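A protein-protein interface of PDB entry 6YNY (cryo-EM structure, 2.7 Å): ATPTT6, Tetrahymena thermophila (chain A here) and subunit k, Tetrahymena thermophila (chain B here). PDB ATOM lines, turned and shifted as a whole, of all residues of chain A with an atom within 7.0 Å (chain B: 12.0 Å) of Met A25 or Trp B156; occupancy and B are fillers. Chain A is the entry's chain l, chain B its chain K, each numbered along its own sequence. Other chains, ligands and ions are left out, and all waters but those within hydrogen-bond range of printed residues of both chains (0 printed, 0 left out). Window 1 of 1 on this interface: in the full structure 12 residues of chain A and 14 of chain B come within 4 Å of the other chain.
The side-chain amide oxygen (OD1) of Asn A28 is in hydrogen-bond range of the side-chain amino group (NZ) of Lys B162 (3.4 Å). The guanidinium group (NE) of Arg B106 lies within salt-bridge range of the side-chain carboxylate (OE2) of Glu A30 (3.2 Å). N of Trp B156 lies within hydrogen-bond range of SD of Met A25.
O of Ser B155 sits at hydrogen-bond distance from NH2 of Arg B106, 2.6 Å away. NE2 of Gln B149 lies close to NH1 of Arg B106. O of Met B157 is in hydrogen-bond range of NZ of Lys B162, 3.2 Å away. The guanidinium group of Arg B106 lies close to the side-chain sulfur of Met B157. The guanidinium group of Arg B106 lies within salt-bridge range of the side-chain carboxylate of Asp B154. The backbone NH (N) of Val B107 is in hydrogen-bond range of the side-chain amide oxygen (OD1) of Asn B105, 2.6 Å away.
Among the printed residues, merely in contact across the chains: Lys A24 with Trp B156, Met A25 with Ser B155, Asn A28 with Arg B106, Asn A28 with Trp B156, Asn A28 with Met B157 and Glu A30 with Asn B105.
Met A25 touches just these residues of chain B: Ser B155 and Trp B156. Asp A22 touches none of the printed residues of chain B. No residue of chain B comes within 4 Å of Asp A23. Of chain B, only Trp B156 comes within 4 Å of Lys A24. Ile A26 touches none of the printed residues of chain B. No residue of chain B comes within 4 Å of Ser A27. Asn A28 touches four residues of chain B. No residue of chain B comes within 4 Å of Ile A29. Of the printed residues of chain A, Lys B162 touches Asn A28 (3.4 Å). Of the printed residues of chain A, Met B157 touches Asn A28. Printed residues of chain A within 4 Å of Arg B106: Asn A28 (3.4 Å) and Glu A30 (3.2 Å). Printed residues of chain B within 4 Å of Glu A30: Asn B105 and Arg B106. Lys B160 touches none of the printed residues of chain A. The nearest residue of chain B that does not touch Met A25 is Asp B154 (5.1 Å). The nearest residue of chain A that does not touch Trp B156 is Tyr A21 (4.3 Å). The nearest printed residue of chain A that does not touch Met B157 is Lys A24 (6.0 Å).
Of the 12 printed residues of chain A, 4 touch a printed residue of chain B. Hydrophobic or aromatic side chains of chain A that line the printed part of chain B: Met A25. Of the 20 printed residues of chain B, 6 touch a printed residue of chain A. Hydrophobic or aromatic side chains of chain B that line the printed part of chain A: Trp B156. Among the printed residues, Asp or Glu carboxylates within 4 Å of a Lys or Arg side-chain nitrogen of the other chain: Glu A30 with Arg B106 (3.2 Å).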
ATOM      1  N   ASP A  19     -18.560   5.018   6.964  1.00  0.00           N
ATOM      2  CA  ASP A  19     -18.917   6.424   6.832  1.00  0.00           C
ATOM      3  C   ASP A  19     -18.725   7.162   8.148  1.00  0.00           C
ATOM      4  O   ASP A  19     -18.322   8.331   8.162  1.00  0.00           O
ATOM      5  CB  ASP A  19     -20.358   6.551   6.348  1.00  0.00           C
ATOM      6  CG  ASP A  19     -20.556   5.982   4.960  1.00  0.00           C
ATOM      7  OD1 ASP A  19     -19.600   6.022   4.158  1.00  0.00           O
ATOM      8  OD2 ASP A  19     -21.668   5.495   4.668  1.00  0.00           O
ATOM      9  N   ALA A  20     -19.006   6.496   9.269  1.00  0.00           N
ATOM     10  CA  ALA A  20     -18.747   7.103  10.567  1.00  0.00           C
ATOM     11  C   ALA A  20     -17.258   7.296  10.804  1.00  0.00           C
ATOM     12  O   ALA A  20     -16.858   8.249  11.483  1.00  0.00           O
ATOM     13  CB  ALA A  20     -19.346   6.246  11.677  1.00  0.00           C
ATOM     14  N   TYR A  21     -16.428   6.408  10.260  1.00  0.00           N
ATOM     15  CA  TYR A  21     -14.987   6.550  10.424  1.00  0.00           C
ATOM     16  C   TYR A  21     -14.449   7.695   9.577  1.00  0.00           C
ATOM     17  O   TYR A  21     -13.562   8.436  10.015  1.00  0.00           O
ATOM     18  CB  TYR A  21     -14.293   5.241  10.062  1.00  0.00           C
ATOM     19  CG  TYR A  21     -12.787   5.316  10.104  1.00  0.00           C
ATOM     20  CD1 TYR A  21     -12.098   5.147  11.293  1.00  0.00           C
ATOM     21  CD2 TYR A  21     -12.056   5.555   8.953  1.00  0.00           C
ATOM     22  CE1 TYR A  21     -10.724   5.217  11.333  1.00  0.00           C
ATOM     23  CE2 TYR A  21     -10.684   5.626   8.985  1.00  0.00           C
ATOM     24  CZ  TYR A  21     -10.023   5.456  10.176  1.00  0.00           C
ATOM     25  OH  TYR A  21      -8.652   5.527  10.212  1.00  0.00           O
ATOM     26  N   ASP A  22     -14.974   7.858   8.362  1.00  0.00           N
ATOM     27  CA  ASP A  22     -14.545   8.967   7.520  1.00  0.00           C
ATOM     28  C   ASP A  22     -14.957  10.300   8.127  1.00  0.00           C
ATOM     29  O   ASP A  22     -14.136  11.214   8.259  1.00  0.00           O
ATOM     30  CB  ASP A  22     -15.126   8.809   6.118  1.00  0.00           C
ATOM     31  CG  ASP A  22     -14.610   7.576   5.411  1.00  0.00           C
ATOM     32  OD1 ASP A  22     -15.097   6.468   5.713  1.00  0.00           O
ATOM     33  OD2 ASP A  22     -13.711   7.709   4.556  1.00  0.00           O
ATOM     34  N   ASP A  23     -16.229  10.431   8.505  1.00  0.00           N
ATOM     35  CA  ASP A  23     -16.672  11.647   9.175  1.00  0.00           C
ATOM     36  C   ASP A  23     -15.898  11.879  10.462  1.00  0.00           C
ATOM     37  O   ASP A  23     -15.660  13.027  10.850  1.00  0.00           O
ATOM     38  CB  ASP A  23     -18.168  11.565   9.464  1.00  0.00           C
ATOM     39  CG  ASP A  23     -18.989  11.316   8.218  1.00  0.00           C
ATOM     40  OD1 ASP A  23     -18.570  11.760   7.130  1.00  0.00           O
ATOM     41  OD2 ASP A  23     -20.055  10.676   8.325  1.00  0.00           O
ATOM     42  N   LYS A  24     -15.498  10.801  11.133  1.00  0.00           N
ATOM     43  CA  LYS A  24     -14.688  10.922  12.337  1.00  0.00           C
ATOM     44  C   LYS A  24     -13.320  11.508  12.016  1.00  0.00           C
ATOM     45  O   LYS A  24     -12.870  12.458  12.667  1.00  0.00           O
ATOM     46  CB  LYS A  24     -14.555   9.554  12.997  1.00  0.00           C
ATOM     47  CG  LYS A  24     -13.783   9.537  14.286  1.00  0.00           C
ATOM     48  CD  LYS A  24     -13.450   8.114  14.673  1.00  0.00           C
ATOM     49  CE  LYS A  24     -13.044   8.017  16.120  1.00  0.00           C
ATOM     50  NZ  LYS A  24     -12.556   6.658  16.453  1.00  0.00           N
ATOM     51  N   MET A  25     -12.641  10.950  11.015  1.00  0.00           N
ATOM     52  CA  MET A  25     -11.324  11.455  10.649  1.00  0.00           C
ATOM     53  C   MET A  25     -11.426  12.821   9.987  1.00  0.00           C
ATOM     54  O   MET A  25     -10.567  13.685  10.196  1.00  0.00           O
ATOM     55  CB  MET A  25     -10.633  10.465   9.715  1.00  0.00           C
ATOM     56  CG  MET A  25      -9.222  10.858   9.335  1.00  0.00           C
ATOM     57  SD  MET A  25      -8.074  10.755  10.713  1.00  0.00           S
ATOM     58  CE  MET A  25      -7.780   8.997  10.721  1.00  0.00           C
ATOM     59  N   ILE A  26     -12.467  13.034   9.183  1.00  0.00           N
ATOM     60  CA  ILE A  26     -12.604  14.297   8.473  1.00  0.00           C
ATOM     61  C   ILE A  26     -12.884  15.434   9.444  1.00  0.00           C
ATOM     62  O   ILE A  26     -12.527  16.587   9.182  1.00  0.00           O
ATOM     63  CB  ILE A  26     -13.701  14.176   7.403  1.00  0.00           C
ATOM     64  CG1 ILE A  26     -13.224  13.268   6.270  1.00  0.00           C
ATOM     65  CG2 ILE A  26     -14.075  15.537   6.875  1.00  0.00           C
ATOM     66  CD1 ILE A  26     -14.305  12.888   5.296  1.00  0.00           C
ATOM     67  N   SER A  27     -13.527  15.137  10.573  1.00  0.00           N
ATOM     68  CA  SER A  27     -13.824  16.165  11.560  1.00  0.00           C
ATOM     69  C   SER A  27     -12.582  16.652  12.292  1.00  0.00           C
ATOM     70  O   SER A  27     -12.635  17.704  12.937  1.00  0.00           O
ATOM     71  CB  SER A  27     -14.841  15.645  12.571  1.00  0.00           C
ATOM     72  OG  SER A  27     -14.329  14.541  13.293  1.00  0.00           O
ATOM     73  N   ASN A  28     -11.475  15.920  12.213  1.00  0.00           N
ATOM     74  CA  ASN A  28     -10.243  16.294  12.890  1.00  0.00           C
ATOM     75  C   ASN A  28      -9.223  16.938  11.963  1.00  0.00           C
ATOM     76  O   ASN A  28      -8.137  17.303  12.422  1.00  0.00           O
ATOM     77  CB  ASN A  28      -9.619  15.068  13.559  1.00  0.00           C
ATOM     78  CG  ASN A  28     -10.423  14.577  14.737  1.00  0.00           C
ATOM     79  OD1 ASN A  28     -10.341  15.126  15.835  1.00  0.00           O
ATOM     80  ND2 ASN A  28     -11.202  13.529  14.522  1.00  0.00           N
ATOM     81  N   ILE A  29      -9.539  17.086  10.680  1.00  0.00           N
ATOM     82  CA  ILE A  29      -8.593  17.671   9.741  1.00  0.00           C
ATOM     83  C   ILE A  29      -8.462  19.162  10.015  1.00  0.00           C
ATOM     84  O   ILE A  29      -9.461  19.873  10.181  1.00  0.00           O
ATOM     85  CB  ILE A  29      -9.035  17.406   8.296  1.00  0.00           C
ATOM     86  CG1 ILE A  29      -9.002  15.908   8.010  1.00  0.00           C
ATOM     87  CG2 ILE A  29      -8.147  18.151   7.326  1.00  0.00           C
ATOM     88  CD1 ILE A  29      -9.432  15.539   6.625  1.00  0.00           C
ATOM     89  N   GLU A  30      -7.222  19.640  10.063  1.00  0.00           N
ATOM     90  CA  GLU A  30      -6.911  21.059  10.212  1.00  0.00           C
ATOM     91  C   GLU A  30      -6.136  21.479   8.969  1.00  0.00           C
ATOM     92  O   GLU A  30      -4.938  21.205   8.854  1.00  0.00           O
ATOM     93  CB  GLU A  30      -6.109  21.322  11.482  1.00  0.00           C
ATOM     94  CG  GLU A  30      -6.803  20.906  12.762  1.00  0.00           C
ATOM     95  CD  GLU A  30      -5.967  21.189  13.994  1.00  0.00           C
ATOM     96  OE1 GLU A  30      -4.928  21.870  13.865  1.00  0.00           O
ATOM     97  OE2 GLU A  30      -6.344  20.730  15.092  1.00  0.00           O
ATOM     98  N   ASN B 105      -7.750  24.778  18.243  1.00  0.00           N
ATOM     99  CA  ASN B 105      -7.500  23.526  17.547  1.00  0.00           C
ATOM    100  C   ASN B 105      -8.110  22.387  18.358  1.00  0.00           C
ATOM    101  O   ASN B 105      -8.873  22.603  19.303  1.00  0.00           O
ATOM    102  CB  ASN B 105      -6.005  23.339  17.304  1.00  0.00           C
ATOM    103  CG  ASN B 105      -5.271  22.845  18.522  1.00  0.00           C
ATOM    104  OD1 ASN B 105      -5.362  21.673  18.884  1.00  0.00           O
ATOM    105  ND2 ASN B 105      -4.514  23.728  19.151  1.00  0.00           N
ATOM    106  N   ARG B 106      -7.780  21.148  17.994  1.00  0.00           N
ATOM    107  CA  ARG B 106      -8.362  19.997  18.670  1.00  0.00           C
ATOM    108  C   ARG B 106      -8.123  20.034  20.171  1.00  0.00           C
ATOM    109  O   ARG B 106      -8.844  19.365  20.920  1.00  0.00           O
ATOM    110  CB  ARG B 106      -7.811  18.717  18.055  1.00  0.00           C
ATOM    111  CG  ARG B 106      -8.334  18.476  16.655  1.00  0.00           C
ATOM    112  CD  ARG B 106      -7.670  17.297  15.982  1.00  0.00           C
ATOM    113  NE  ARG B 106      -6.266  17.546  15.690  1.00  0.00           N
ATOM    114  CZ  ARG B 106      -5.478  16.686  15.060  1.00  0.00           C
ATOM    115  NH1 ARG B 106      -4.212  16.992  14.831  1.00  0.00           N
ATOM    116  NH2 ARG B 106      -5.957  15.518  14.660  1.00  0.00           N
ATOM    117  N   VAL B 107      -7.134  20.794  20.624  1.00  0.00           N
ATOM    118  CA  VAL B 107      -6.983  21.127  22.031  1.00  0.00           C
ATOM    119  C   VAL B 107      -7.322  22.604  22.190  1.00  0.00           C
ATOM    120  O   VAL B 107      -7.269  23.390  21.241  1.00  0.00           O
ATOM    121  CB  VAL B 107      -5.570  20.822  22.569  1.00  0.00           C
ATOM    122  CG1 VAL B 107      -5.146  19.424  22.186  1.00  0.00           C
ATOM    123  CG2 VAL B 107      -4.572  21.833  22.060  1.00  0.00           C
ATOM    124  N   HIS B 141       5.439  17.079  25.282  1.00  0.00           N
ATOM    125  CA  HIS B 141       4.788  16.062  24.467  1.00  0.00           C
ATOM    126  C   HIS B 141       3.875  16.686  23.420  1.00  0.00           C
ATOM    127  O   HIS B 141       3.872  16.260  22.260  1.00  0.00           O
ATOM    128  CB  HIS B 141       3.999  15.111  25.360  1.00  0.00           C
ATOM    129  CG  HIS B 141       3.271  14.044  24.606  1.00  0.00           C
ATOM    130  ND1 HIS B 141       3.916  13.130  23.803  1.00  0.00           N
ATOM    131  CD2 HIS B 141       1.953  13.753  24.526  1.00  0.00           C
ATOM    132  CE1 HIS B 141       3.025  12.318  23.264  1.00  0.00           C
ATOM    133  NE2 HIS B 141       1.826  12.674  23.686  1.00  0.00           N
ATOM    134  N   VAL B 145       4.066  16.068  19.338  1.00  0.00           N
ATOM    135  CA  VAL B 145       2.980  15.651  18.456  1.00  0.00           C
ATOM    136  C   VAL B 145       2.877  16.596  17.268  1.00  0.00           C
ATOM    137  O   VAL B 145       2.829  16.166  16.110  1.00  0.00           O
ATOM    138  CB  VAL B 145       1.655  15.587  19.234  1.00  0.00           C
ATOM    139  CG1 VAL B 145       0.520  15.235  18.305  1.00  0.00           C
ATOM    140  CG2 VAL B 145       1.747  14.589  20.361  1.00  0.00           C
ATOM    141  N   ASP B 148       5.276  16.085  14.712  1.00  0.00           N
ATOM    142  CA  ASP B 148       4.951  14.943  13.868  1.00  0.00           C
ATOM    143  C   ASP B 148       3.840  15.269  12.881  1.00  0.00           C
ATOM    144  O   ASP B 148       3.848  14.762  11.755  1.00  0.00           O
ATOM    145  CB  ASP B 148       4.544  13.754  14.734  1.00  0.00           C
ATOM    146  CG  ASP B 148       5.700  13.192  15.528  1.00  0.00           C
ATOM    147  OD1 ASP B 148       6.500  13.988  16.060  1.00  0.00           O
ATOM    148  OD2 ASP B 148       5.804  11.954  15.630  1.00  0.00           O
ATOM    149  N   GLN B 149       2.881  16.103  13.285  1.00  0.00           N
ATOM    150  CA  GLN B 149       1.831  16.526  12.367  1.00  0.00           C
ATOM    151  C   GLN B 149       2.416  17.256  11.169  1.00  0.00           C
ATOM    152  O   GLN B 149       1.987  17.044  10.029  1.00  0.00           O
ATOM    153  CB  GLN B 149       0.839  17.427  13.093  1.00  0.00           C
ATOM    154  CG  GLN B 149       0.121  16.772  14.246  1.00  0.00           C
ATOM    155  CD  GLN B 149      -0.652  17.765  15.080  1.00  0.00           C
ATOM    156  OE1 GLN B 149      -0.453  18.973  14.971  1.00  0.00           O
ATOM    157  NE2 GLN B 149      -1.544  17.263  15.919  1.00  0.00           N
ATOM    158  N   GLY B 152       3.632  14.881   8.559  1.00  0.00           N
ATOM    159  CA  GLY B 152       2.630  14.108   7.849  1.00  0.00           C
ATOM    160  C   GLY B 152       1.939  13.046   8.674  1.00  0.00           C
ATOM    161  O   GLY B 152       1.103  12.316   8.126  1.00  0.00           O
ATOM    162  N   LEU B 153       2.241  12.912   9.959  1.00  0.00           N
ATOM    163  CA  LEU B 153       1.623  11.905  10.810  1.00  0.00           C
ATOM    164  C   LEU B 153       0.549  12.573  11.657  1.00  0.00           C
ATOM    165  O   LEU B 153       0.859  13.303  12.604  1.00  0.00           O
ATOM    166  CB  LEU B 153       2.665  11.223  11.690  1.00  0.00           C
ATOM    167  CG  LEU B 153       2.150  10.085  12.564  1.00  0.00           C
ATOM    168  CD1 LEU B 153       1.655   8.947  11.705  1.00  0.00           C
ATOM    169  CD2 LEU B 153       3.229   9.615  13.501  1.00  0.00           C
ATOM    170  N   ASP B 154      -0.710  12.322  11.318  1.00  0.00           N
ATOM    171  CA  ASP B 154      -1.826  12.864  12.071  1.00  0.00           C
ATOM    172  C   ASP B 154      -2.970  11.867  12.007  1.00  0.00           C
ATOM    173  O   ASP B 154      -3.007  10.989  11.143  1.00  0.00           O
ATOM    174  CB  ASP B 154      -2.260  14.230  11.539  1.00  0.00           C
ATOM    175  CG  ASP B 154      -3.241  14.926  12.452  1.00  0.00           C
ATOM    176  OD1 ASP B 154      -3.604  14.340  13.492  1.00  0.00           O
ATOM    177  OD2 ASP B 154      -3.646  16.063  12.136  1.00  0.00           O
ATOM    178  N   SER B 155      -3.903  12.010  12.938  1.00  0.00           N
ATOM    179  CA  SER B 155      -5.041  11.109  13.025  1.00  0.00           C
ATOM    180  C   SER B 155      -6.121  11.788  13.853  1.00  0.00           C
ATOM    181  O   SER B 155      -6.039  12.982  14.157  1.00  0.00           O
ATOM    182  CB  SER B 155      -4.626   9.766  13.626  1.00  0.00           C
ATOM    183  OG  SER B 155      -5.714   8.864  13.657  1.00  0.00           O
ATOM    184  N   TRP B 156      -7.142  11.022  14.211  1.00  0.00           N
ATOM    185  CA  TRP B 156      -8.216  11.534  15.042  1.00  0.00           C
ATOM    186  C   TRP B 156      -7.820  11.469  16.509  1.00  0.00           C
ATOM    187  O   TRP B 156      -6.977  10.663  16.913  1.00  0.00           O
ATOM    188  CB  TRP B 156      -9.500  10.742  14.803  1.00  0.00           C
ATOM    189  CG  TRP B 156      -9.365   9.285  15.072  1.00  0.00           C
ATOM    190  CD1 TRP B 156      -9.003   8.323  14.183  1.00  0.00           C
ATOM    191  CD2 TRP B 156      -9.588   8.619  16.316  1.00  0.00           C
ATOM    192  NE1 TRP B 156      -8.986   7.097  14.793  1.00  0.00           N
ATOM    193  CE2 TRP B 156      -9.343   7.252  16.105  1.00  0.00           C
ATOM    194  CE3 TRP B 156      -9.974   9.046  17.588  1.00  0.00           C
ATOM    195  CZ2 TRP B 156      -9.468   6.309  17.116  1.00  0.00           C
ATOM    196  CZ3 TRP B 156     -10.100   8.109  18.588  1.00  0.00           C
ATOM    197  CH2 TRP B 156      -9.847   6.757  18.348  1.00  0.00           C
ATOM    198  N   MET B 157      -8.431  12.336  17.305  1.00  0.00           N
ATOM    199  CA  MET B 157      -8.138  12.448  18.723  1.00  0.00           C
ATOM    200  C   MET B 157      -9.364  12.074  19.539  1.00  0.00           C
ATOM    201  O   MET B 157     -10.489  12.441  19.191  1.00  0.00           O
ATOM    202  CB  MET B 157      -7.692  13.865  19.074  1.00  0.00           C
ATOM    203  CG  MET B 157      -6.393  14.268  18.424  1.00  0.00           C
ATOM    204  SD  MET B 157      -5.956  15.990  18.695  1.00  0.00           S
ATOM    205  CE  MET B 157      -5.779  15.998  20.468  1.00  0.00           C
ATOM    206  N   SER B 158      -9.137  11.338  20.622  1.00  0.00           N
ATOM    207  CA  SER B 158     -10.204  10.975  21.535  1.00  0.00           C
ATOM    208  C   SER B 158     -10.466  12.115  22.513  1.00  0.00           C
ATOM    209  O   SER B 158      -9.780  13.141  22.519  1.00  0.00           O
ATOM    210  CB  SER B 158      -9.845   9.693  22.277  1.00  0.00           C
ATOM    211  OG  SER B 158      -8.644   9.849  23.008  1.00  0.00           O
ATOM    212  N   GLU B 159     -11.479  11.933  23.359  1.00  0.00           N
ATOM    213  CA  GLU B 159     -11.790  12.947  24.358  1.00  0.00           C
ATOM    214  C   GLU B 159     -10.676  13.075  25.383  1.00  0.00           C
ATOM    215  O   GLU B 159     -10.483  14.153  25.957  1.00  0.00           O
ATOM    216  CB  GLU B 159     -13.109  12.615  25.051  1.00  0.00           C
ATOM    217  CG  GLU B 159     -14.287  12.473  24.103  1.00  0.00           C
ATOM    218  CD  GLU B 159     -14.582  13.749  23.338  1.00  0.00           C
ATOM    219  OE1 GLU B 159     -14.042  14.810  23.715  1.00  0.00           O
ATOM    220  OE2 GLU B 159     -15.355  13.690  22.359  1.00  0.00           O
ATOM    221  N   LYS B 160      -9.936  11.995  25.627  1.00  0.00           N
ATOM    222  CA  LYS B 160      -8.837  12.051  26.581  1.00  0.00           C
ATOM    223  C   LYS B 160      -7.609  12.711  25.971  1.00  0.00           C
ATOM    224  O   LYS B 160      -6.911  13.474  26.647  1.00  0.00           O
ATOM    225  CB  LYS B 160      -8.508  10.644  27.068  1.00  0.00           C
ATOM    226  CG  LYS B 160      -7.574  10.601  28.261  1.00  0.00           C
ATOM    227  CD  LYS B 160      -7.363   9.180  28.756  1.00  0.00           C
ATOM    228  CE  LYS B 160      -8.607   8.613  29.419  1.00  0.00           C
ATOM    229  NZ  LYS B 160      -9.038   9.419  30.594  1.00  0.00           N
ATOM    230  N   ASP B 161      -7.326  12.429  24.698  1.00  0.00           N
ATOM    231  CA  ASP B 161      -6.220  13.101  24.030  1.00  0.00           C
ATOM    232  C   ASP B 161      -6.489  14.590  23.877  1.00  0.00           C
ATOM    233  O   ASP B 161      -5.558  15.399  23.958  1.00  0.00           O
ATOM    234  CB  ASP B 161      -5.971  12.473  22.660  1.00  0.00           C
ATOM    235  CG  ASP B 161      -5.511  11.036  22.750  1.00  0.00           C
ATOM    236  OD1 ASP B 161      -4.828  10.688  23.734  1.00  0.00           O
ATOM    237  OD2 ASP B 161      -5.829  10.254  21.830  1.00  0.00           O
ATOM    238  N   LYS B 162      -7.748  14.970  23.656  1.00  0.00           N
ATOM    239  CA  LYS B 162      -8.092  16.376  23.497  1.00  0.00           C
ATOM    240  C   LYS B 162      -7.803  17.194  24.746  1.00  0.00           C
ATOM    241  O   LYS B 162      -7.646  18.416  24.649  1.00  0.00           O
ATOM    242  CB  LYS B 162      -9.566  16.514  23.132  1.00  0.00           C
ATOM    243  CG  LYS B 162      -9.867  16.316  21.664  1.00  0.00           C
ATOM    244  CD  LYS B 162     -11.338  16.542  21.381  1.00  0.00           C
ATOM    245  CE  LYS B 162     -11.601  16.730  19.902  1.00  0.00           C
ATOM    246  NZ  LYS B 162     -11.164  15.564  19.100  1.00  0.00           N
ATOM    247  N   ASN B 163      -7.733  16.555  25.912  1.00  0.00           N
ATOM    248  CA  ASN B 163      -7.507  17.245  27.175  1.00  0.00           C
ATOM    249  C   ASN B 163      -6.088  17.058  27.695  1.00  0.00           C
ATOM    250  O   ASN B 163      -5.853  17.150  28.903  1.00  0.00           O
ATOM    251  CB  ASN B 163      -8.519  16.771  28.215  1.00  0.00           C
ATOM    252  CG  ASN B 163      -9.944  17.081  27.819  1.00  0.00           C
ATOM    253  OD1 ASN B 163     -10.204  18.044  27.097  1.00  0.00           O
ATOM    254  ND2 ASN B 163     -10.876  16.268  28.288  1.00  0.00           N
ATOM    255  N   MET B 164      -5.131  16.800  26.801  1.00  0.00           N
ATOM    256  CA  MET B 164      -3.752  16.612  27.237  1.00  0.00           C
ATOM    257  C   MET B 164      -3.223  17.838  27.964  1.00  0.00           C
ATOM    258  O   MET B 164      -2.383  17.712  28.861  1.00  0.00           O
ATOM    259  CB  MET B 164      -2.858  16.296  26.038  1.00  0.00           C
ATOM    260  CG  MET B 164      -2.807  17.383  24.987  1.00  0.00           C
ATOM    261  SD  MET B 164      -1.477  17.144  23.799  1.00  0.00           S
ATOM    262  CE  MET B 164      -1.900  15.536  23.152  1.00  0.00           C
